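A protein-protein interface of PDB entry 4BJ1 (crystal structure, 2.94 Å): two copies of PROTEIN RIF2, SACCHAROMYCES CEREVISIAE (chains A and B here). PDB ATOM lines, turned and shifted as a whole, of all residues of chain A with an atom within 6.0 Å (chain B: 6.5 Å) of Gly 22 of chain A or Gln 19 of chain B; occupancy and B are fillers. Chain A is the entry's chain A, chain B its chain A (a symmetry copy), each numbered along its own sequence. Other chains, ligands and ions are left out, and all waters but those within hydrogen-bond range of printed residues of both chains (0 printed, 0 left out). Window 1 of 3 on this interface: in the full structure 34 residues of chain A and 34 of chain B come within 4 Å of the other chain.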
ATOM      1  N   ALA A  17      -7.286  23.515   8.711  1.00  0.00           N
ATOM      2  CA  ALA A  17      -8.447  23.960   9.467  1.00  0.00           C
ATOM      3  C   ALA A  17      -8.071  23.937  10.945  1.00  0.00           C
ATOM      4  O   ALA A  17      -8.337  24.906  11.650  1.00  0.00           O
ATOM      5  CB  ALA A  17      -9.649  23.060   9.196  1.00  0.00           C
ATOM      6  N   LEU A  18      -7.391  22.879  11.402  1.00  0.00           N
ATOM      7  CA  LEU A  18      -6.957  22.791  12.784  1.00  0.00           C
ATOM      8  C   LEU A  18      -6.012  23.909  13.171  1.00  0.00           C
ATOM      9  O   LEU A  18      -6.269  24.581  14.176  1.00  0.00           O
ATOM     10  CB  LEU A  18      -6.392  21.426  13.104  1.00  0.00           C
ATOM     11  CG  LEU A  18      -7.481  20.468  13.531  1.00  0.00           C
ATOM     12  CD1 LEU A  18      -7.243  19.082  13.001  1.00  0.00           C
ATOM     13  CD2 LEU A  18      -7.667  20.487  15.050  1.00  0.00           C
ATOM     14  N   GLN A  19      -5.016  24.215  12.313  1.00  0.00           N
ATOM     15  CA  GLN A  19      -4.107  25.339  12.545  1.00  0.00           C
ATOM     16  C   GLN A  19      -4.845  26.683  12.512  1.00  0.00           C
ATOM     17  O   GLN A  19      -4.617  27.485  13.413  1.00  0.00           O
ATOM     18  CB  GLN A  19      -2.997  25.338  11.525  1.00  0.00           C
ATOM     19  CG  GLN A  19      -1.870  26.286  11.856  1.00  0.00           C
ATOM     20  CD  GLN A  19      -1.277  26.799  10.587  1.00  0.00           C
ATOM     21  OE1 GLN A  19      -1.977  27.035   9.604  1.00  0.00           O
ATOM     22  NE2 GLN A  19       0.028  26.956  10.561  1.00  0.00           N
ATOM     23  N   GLU A  20      -5.772  26.908  11.538  1.00  0.00           N
ATOM     24  CA  GLU A  20      -6.480  28.182  11.489  1.00  0.00           C
ATOM     25  C   GLU A  20      -7.411  28.380  12.646  1.00  0.00           C
ATOM     26  O   GLU A  20      -7.462  29.485  13.167  1.00  0.00           O
ATOM     27  CB  GLU A  20      -7.197  28.454  10.169  1.00  0.00           C
ATOM     28  CG  GLU A  20      -7.368  29.960  10.001  1.00  0.00           C
ATOM     29  CD  GLU A  20      -7.867  30.556   8.702  1.00  0.00           C
ATOM     30  OE1 GLU A  20      -8.085  29.789   7.742  1.00  0.00           O
ATOM     31  OE2 GLU A  20      -8.066  31.793   8.653  1.00  0.00           O
ATOM     32  N   LEU A  21      -8.135  27.325  13.074  1.00  0.00           N
ATOM     33  CA  LEU A  21      -9.047  27.403  14.216  1.00  0.00           C
ATOM     34  C   LEU A  21      -8.204  27.775  15.457  1.00  0.00           C
ATOM     35  O   LEU A  21      -8.565  28.715  16.169  1.00  0.00           O
ATOM     36  CB  LEU A  21      -9.829  26.078  14.361  1.00  0.00           C
ATOM     37  CG  LEU A  21     -11.004  26.009  15.359  1.00  0.00           C
ATOM     38  CD1 LEU A  21     -12.160  26.962  14.984  1.00  0.00           C
ATOM     39  CD2 LEU A  21     -11.535  24.599  15.424  1.00  0.00           C
ATOM     40  N   GLY A  22      -7.017  27.158  15.582  1.00  0.00           N
ATOM     41  CA  GLY A  22      -6.052  27.481  16.625  1.00  0.00           C
ATOM     42  C   GLY A  22      -5.688  28.953  16.614  1.00  0.00           C
ATOM     43  O   GLY A  22      -5.885  29.659  17.603  1.00  0.00           O
ATOM     44  N   THR A  23      -5.240  29.439  15.462  1.00  0.00           N
ATOM     45  CA  THR A  23      -4.896  30.841  15.191  1.00  0.00           C
ATOM     46  C   THR A  23      -6.056  31.805  15.460  1.00  0.00           C
ATOM     47  O   THR A  23      -5.849  32.826  16.118  1.00  0.00           O
ATOM     48  CB  THR A  23      -4.369  30.937  13.761  1.00  0.00           C
ATOM     49  OG1 THR A  23      -3.172  30.175  13.711  1.00  0.00           O
ATOM     50  CG2 THR A  23      -4.081  32.342  13.328  1.00  0.00           C
ATOM     51  N   ASN A  24      -7.253  31.483  14.949  1.00  0.00           N
ATOM     52  CA  ASN A  24      -8.474  32.265  15.116  1.00  0.00           C
ATOM     53  C   ASN A  24      -8.798  32.474  16.573  1.00  0.00           C
ATOM     54  O   ASN A  24      -9.020  33.610  16.949  1.00  0.00           O
ATOM     55  CB  ASN A  24      -9.660  31.631  14.380  1.00  0.00           C
ATOM     56  CG  ASN A  24      -9.602  31.775  12.885  1.00  0.00           C
ATOM     57  OD1 ASN A  24      -8.742  32.448  12.323  1.00  0.00           O
ATOM     58  ND2 ASN A  24     -10.514  31.138  12.200  1.00  0.00           N
ATOM     59  N   TYR A  25      -8.778  31.409  17.394  1.00  0.00           N
ATOM     60  CA  TYR A  25      -8.998  31.477  18.837  1.00  0.00           C
ATOM     61  C   TYR A  25      -7.997  32.427  19.483  1.00  0.00           C
ATOM     62  O   TYR A  25      -8.409  33.340  20.202  1.00  0.00           O
ATOM     63  CB  TYR A  25      -8.825  30.084  19.448  1.00  0.00           C
ATOM     64  CG  TYR A  25      -9.115  29.954  20.930  1.00  0.00           C
ATOM     65  CD1 TYR A  25     -10.417  29.770  21.388  1.00  0.00           C
ATOM     66  CD2 TYR A  25      -8.077  29.827  21.857  1.00  0.00           C
ATOM     67  CE1 TYR A  25     -10.688  29.556  22.739  1.00  0.00           C
ATOM     68  CE2 TYR A  25      -8.334  29.579  23.208  1.00  0.00           C
ATOM     69  CZ  TYR A  25      -9.646  29.459  23.646  1.00  0.00           C
ATOM     70  OH  TYR A  25      -9.939  29.230  24.971  1.00  0.00           O
ATOM     71  N   LEU A  26      -6.694  32.252  19.187  1.00  0.00           N
ATOM     72  CA  LEU A  26      -5.628  33.067  19.788  1.00  0.00           C
ATOM     73  C   LEU A  26      -5.530  34.510  19.272  1.00  0.00           C
ATOM     74  O   LEU A  26      -4.696  35.286  19.767  1.00  0.00           O
ATOM     75  CB  LEU A  26      -4.271  32.369  19.652  1.00  0.00           C
ATOM     76  CG  LEU A  26      -4.174  30.957  20.179  1.00  0.00           C
ATOM     77  CD1 LEU A  26      -2.891  30.311  19.701  1.00  0.00           C
ATOM     78  CD2 LEU A  26      -4.343  30.903  21.701  1.00  0.00           C
ATOM     79  N   SER A  27      -6.374  34.870  18.293  1.00  0.00           N
ATOM     80  CA  SER A  27      -6.421  36.196  17.683  1.00  0.00           C
ATOM     81  C   SER A  27      -6.868  37.259  18.678  1.00  0.00           C
ATOM     82  O   SER A  27      -7.779  37.016  19.486  1.00  0.00           O
ATOM     83  CB  SER A  27      -7.337  36.183  16.464  1.00  0.00           C
ATOM     84  OG  SER A  27      -7.675  37.479  15.997  1.00  0.00           O
ATOM     85  N   ARG A  66      -0.130  34.785  23.824  1.00  0.00           N
ATOM     86  CA  ARG A  66       0.479  34.590  22.516  1.00  0.00           C
ATOM     87  C   ARG A  66       1.010  35.914  21.944  1.00  0.00           C
ATOM     88  O   ARG A  66       2.130  35.947  21.440  1.00  0.00           O
ATOM     89  CB  ARG A  66      -0.503  33.923  21.530  1.00  0.00           C
ATOM     90  CG  ARG A  66       0.024  33.771  20.081  1.00  0.00           C
ATOM     91  CD  ARG A  66       1.377  33.071  19.994  1.00  0.00           C
ATOM     92  NE  ARG A  66       1.230  31.637  20.199  1.00  0.00           N
ATOM     93  CZ  ARG A  66       1.394  30.740  19.238  1.00  0.00           C
ATOM     94  NH1 ARG A  66       1.751  31.124  18.020  1.00  0.00           N
ATOM     95  NH2 ARG A  66       1.231  29.446  19.493  1.00  0.00           N
ATOM     96  N   PHE A 281     -14.609  26.254  20.447  1.00  0.00           N
ATOM     97  CA  PHE A 281     -13.306  25.728  20.067  1.00  0.00           C
ATOM     98  C   PHE A 281     -13.242  24.232  20.378  1.00  0.00           C
ATOM     99  O   PHE A 281     -12.906  23.447  19.496  1.00  0.00           O
ATOM    100  CB  PHE A 281     -12.192  26.506  20.791  1.00  0.00           C
ATOM    101  CG  PHE A 281     -10.797  26.088  20.417  1.00  0.00           C
ATOM    102  CD1 PHE A 281     -10.215  26.528  19.229  1.00  0.00           C
ATOM    103  CD2 PHE A 281     -10.067  25.226  21.237  1.00  0.00           C
ATOM    104  CE1 PHE A 281      -8.931  26.116  18.873  1.00  0.00           C
ATOM    105  CE2 PHE A 281      -8.780  24.814  20.876  1.00  0.00           C
ATOM    106  CZ  PHE A 281      -8.223  25.266  19.707  1.00  0.00           C
ATOM    107  N   LYS B  14      -3.574  23.495  25.389  1.00  0.00           N
ATOM    108  CA  LYS B  14      -4.320  22.730  24.399  1.00  0.00           C
ATOM    109  C   LYS B  14      -4.424  23.503  23.101  1.00  0.00           C
ATOM    110  O   LYS B  14      -3.977  22.996  22.070  1.00  0.00           O
ATOM    111  CB  LYS B  14      -5.717  22.392  24.945  1.00  0.00           C
ATOM    112  CG  LYS B  14      -6.585  21.536  24.024  1.00  0.00           C
ATOM    113  CD  LYS B  14      -7.644  20.850  24.840  1.00  0.00           C
ATOM    114  CE  LYS B  14      -8.785  20.348  24.024  1.00  0.00           C
ATOM    115  NZ  LYS B  14      -9.881  19.933  24.923  1.00  0.00           N
ATOM    116  N   SER B  15      -4.987  24.741  23.152  1.00  0.00           N
ATOM    117  CA  SER B  15      -5.194  25.564  21.970  1.00  0.00           C
ATOM    118  C   SER B  15      -3.867  25.925  21.275  1.00  0.00           C
ATOM    119  O   SER B  15      -3.796  25.907  20.039  1.00  0.00           O
ATOM    120  CB  SER B  15      -5.991  26.811  22.329  1.00  0.00           C
ATOM    121  OG  SER B  15      -5.196  27.726  23.062  1.00  0.00           O
ATOM    122  N   MET B  16      -2.821  26.232  22.067  1.00  0.00           N
ATOM    123  CA  MET B  16      -1.512  26.622  21.546  1.00  0.00           C
ATOM    124  C   MET B  16      -0.771  25.429  20.947  1.00  0.00           C
ATOM    125  O   MET B  16      -0.058  25.579  19.940  1.00  0.00           O
ATOM    126  CB  MET B  16      -0.675  27.300  22.637  1.00  0.00           C
ATOM    127  CG  MET B  16      -1.015  28.758  22.848  1.00  0.00           C
ATOM    128  SD  MET B  16       0.085  29.505  24.071  1.00  0.00           S
ATOM    129  CE  MET B  16      -0.566  31.122  24.154  1.00  0.00           C
ATOM    130  N   ALA B  17      -0.931  24.249  21.578  1.00  0.00           N
ATOM    131  CA  ALA B  17      -0.325  22.998  21.142  1.00  0.00           C
ATOM    132  C   ALA B  17      -0.999  22.591  19.836  1.00  0.00           C
ATOM    133  O   ALA B  17      -0.307  22.239  18.885  1.00  0.00           O
ATOM    134  CB  ALA B  17      -0.495  21.915  22.203  1.00  0.00           C
ATOM    135  N   LEU B  18      -2.329  22.708  19.754  1.00  0.00           N
ATOM    136  CA  LEU B  18      -3.050  22.383  18.536  1.00  0.00           C
ATOM    137  C   LEU B  18      -2.629  23.241  17.362  1.00  0.00           C
ATOM    138  O   LEU B  18      -2.292  22.684  16.311  1.00  0.00           O
ATOM    139  CB  LEU B  18      -4.546  22.400  18.753  1.00  0.00           C
ATOM    140  CG  LEU B  18      -5.045  21.059  19.242  1.00  0.00           C
ATOM    141  CD1 LEU B  18      -6.137  21.211  20.264  1.00  0.00           C
ATOM    142  CD2 LEU B  18      -5.463  20.167  18.071  1.00  0.00           C
ATOM    143  N   GLN B  19      -2.497  24.568  17.570  1.00  0.00           N
ATOM    144  CA  GLN B  19      -2.003  25.472  16.529  1.00  0.00           C
ATOM    145  C   GLN B  19      -0.549  25.164  16.150  1.00  0.00           C
ATOM    146  O   GLN B  19      -0.269  25.095  14.957  1.00  0.00           O
ATOM    147  CB  GLN B  19      -2.122  26.906  16.978  1.00  0.00           C
ATOM    148  CG  GLN B  19      -1.903  27.907  15.871  1.00  0.00           C
ATOM    149  CD  GLN B  19      -1.289  29.141  16.444  1.00  0.00           C
ATOM    150  OE1 GLN B  19      -0.468  29.080  17.357  1.00  0.00           O
ATOM    151  NE2 GLN B  19      -1.690  30.290  15.950  1.00  0.00           N
ATOM    152  N   GLU B  20       0.354  24.905  17.137  1.00  0.00           N
ATOM    153  CA  GLU B  20       1.742  24.614  16.795  1.00  0.00           C
ATOM    154  C   GLU B  20       1.906  23.308  16.079  1.00  0.00           C
ATOM    155  O   GLU B  20       2.686  23.257  15.138  1.00  0.00           O
ATOM    156  CB  GLU B  20       2.713  24.712  17.968  1.00  0.00           C
ATOM    157  CG  GLU B  20       4.113  24.984  17.427  1.00  0.00           C
ATOM    158  CD  GLU B  20       5.262  25.326  18.352  1.00  0.00           C
ATOM    159  OE1 GLU B  20       5.027  25.440  19.573  1.00  0.00           O
ATOM    160  OE2 GLU B  20       6.405  25.458  17.856  1.00  0.00           O
ATOM    161  N   LEU B  21       1.172  22.253  16.492  1.00  0.00           N
ATOM    162  CA  LEU B  21       1.234  20.944  15.840  1.00  0.00           C
ATOM    163  C   LEU B  21       0.779  21.135  14.375  1.00  0.00           C
ATOM    164  O   LEU B  21       1.484  20.692  13.465  1.00  0.00           O
ATOM    165  CB  LEU B  21       0.391  19.918  16.632  1.00  0.00           C
ATOM    166  CG  LEU B  21       0.486  18.426  16.256  1.00  0.00           C
ATOM    167  CD1 LEU B  21       1.898  17.843  16.483  1.00  0.00           C
ATOM    168  CD2 LEU B  21      -0.506  17.632  17.069  1.00  0.00           C
ATOM    169  N   GLY B  22      -0.277  21.940  14.175  1.00  0.00           N
ATOM    170  CA  GLY B  22      -0.758  22.318  12.852  1.00  0.00           C
ATOM    171  C   GLY B  22       0.339  22.958  12.022  1.00  0.00           C
ATOM    172  O   GLY B  22       0.684  22.468  10.947  1.00  0.00           O
ATOM    173  N   THR B  23       0.950  24.006  12.562  1.00  0.00           N
ATOM    174  CA  THR B  23       2.082  24.739  11.983  1.00  0.00           C
ATOM    175  C   THR B  23       3.289  23.844  11.687  1.00  0.00           C
ATOM    176  O   THR B  23       3.844  23.924  10.590  1.00  0.00           O
ATOM    177  CB  THR B  23       2.425  25.902  12.912  1.00  0.00           C
ATOM    178  OG1 THR B  23       1.300  26.769  12.920  1.00  0.00           O
ATOM    179  CG2 THR B  23       3.638  26.670  12.479  1.00  0.00           C
ATOM    180  N   ASN B  24       3.687  23.010  12.659  1.00  0.00           N
ATOM    181  CA  ASN B  24       4.799  22.070  12.554  1.00  0.00           C
ATOM    182  C   ASN B  24       4.621  21.134  11.387  1.00  0.00           C
ATOM    183  O   ASN B  24       5.546  21.015  10.606  1.00  0.00           O
ATOM    184  CB  ASN B  24       5.006  21.286  13.855  1.00  0.00           C
ATOM    185  CG  ASN B  24       5.606  22.096  14.970  1.00  0.00           C
ATOM    186  OD1 ASN B  24       6.005  23.245  14.807  1.00  0.00           O
ATOM    187  ND2 ASN B  24       5.678  21.517  16.140  1.00  0.00           N
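O of Gln 19 of chain A is in hydrogen-bond range of OG1 of Thr 23 of chain A (3.1 Å). The backbone carbonyl oxygen (O) of Gln 19 of chain B is in hydrogen-bond range of the side-chain hydroxyl (OG1) of Thr 23 of chain B (3.1 Å).
Hydrophobic or aromatic side chains of chain B within 4 Å of the printed part of chain A: Met 16 and Leu 18.
Of the printed residues of chain B, Leu 18 of chain A touches Leu 18 (3.8 Å). Printed residues of chain B within 4 Å of Gly 22 of chain A: Gln 19 (3.99 Å). Of the printed residues of chain B, Arg 66 of chain A touches Met 16 (3.7 Å) and Gln 19 (2.8 Å). Of the printed residues of chain A, Gln 19 of chain B touches Gln 19, Gly 22, Thr 23, Leu 26 and Arg 66. Printed residues of chain A within 4 Å of Gly 22 of chain B: Gln 19. The nearest printed residue of chain B that does not touch Gly 22 of chain A is Ser 15 of chain B (4.4 Å). The nearest printed residue of chain A that does not touch Gln 19 of chain B is Leu 18 of chain A (5.0 Å). The nearest printed residue of chain A that does not touch Gly 22 of chain B is Leu 18 of chain A (5.5 Å).
Leu 18 of chain B touches its own counterpart, Leu 18 of chain A. Gln 19 of chain A touches its own counterpart, Gln 19 of chain B. Gln 19 of chain A touches Gly 22 of chain B, and with the chains exchanged Gly 22 of chain A touches Gln 19 of chain B. Gln 19 of chain A touches Thr 23 of chain B, and with the chains exchanged Thr 23 of chain A touches Gln 19 of chain B. Positions printed for both chains: 17, 18, 19, 20, 21, 22, 23 and 24.
Leu 18 of chain A touches Leu 18 of chain B (CD2 to CD2, 3.8 Å). Gln 19 of chain A touches Gln 19 of chain B. Gln 19 of chain A touches Gly 22 of chain B (CB to CA, 3.99 Å). CB of Gln 19 of chain B touches CA of Gly 22 of chain A, at 3.99 Å. Ser 15 of chain B touches Tyr 25 of chain A. OG of Ser 15 of chain B touches CD2 of Leu 26 of chain A, 3.6 Å away. Leu 26 of chain A touches Met 16 of chain B. Gln 19 of chain B touches Leu 26 of chain A. Met 16 of chain B touches Arg 66 of chain A (CE to N, 3.7 Å). CE2 of Phe 281 of chain A touches CB of Ser 15 of chain B, 3.7 Å away.
NE2 of Gln 19 of chain A lies within hydrogen-bond range of OG1 of Thr 23 of chain B. The side-chain hydroxyl (OG1) of Thr 23 of chain A is in hydrogen-bond range of the side-chain amide nitrogen (NE2) of Gln 19 of chain B (2.7 Å). NH2 of Arg 66 of chain A lies within hydrogen-bond range of OE1 of Gln 19 of chain B, at 2.8 Å.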
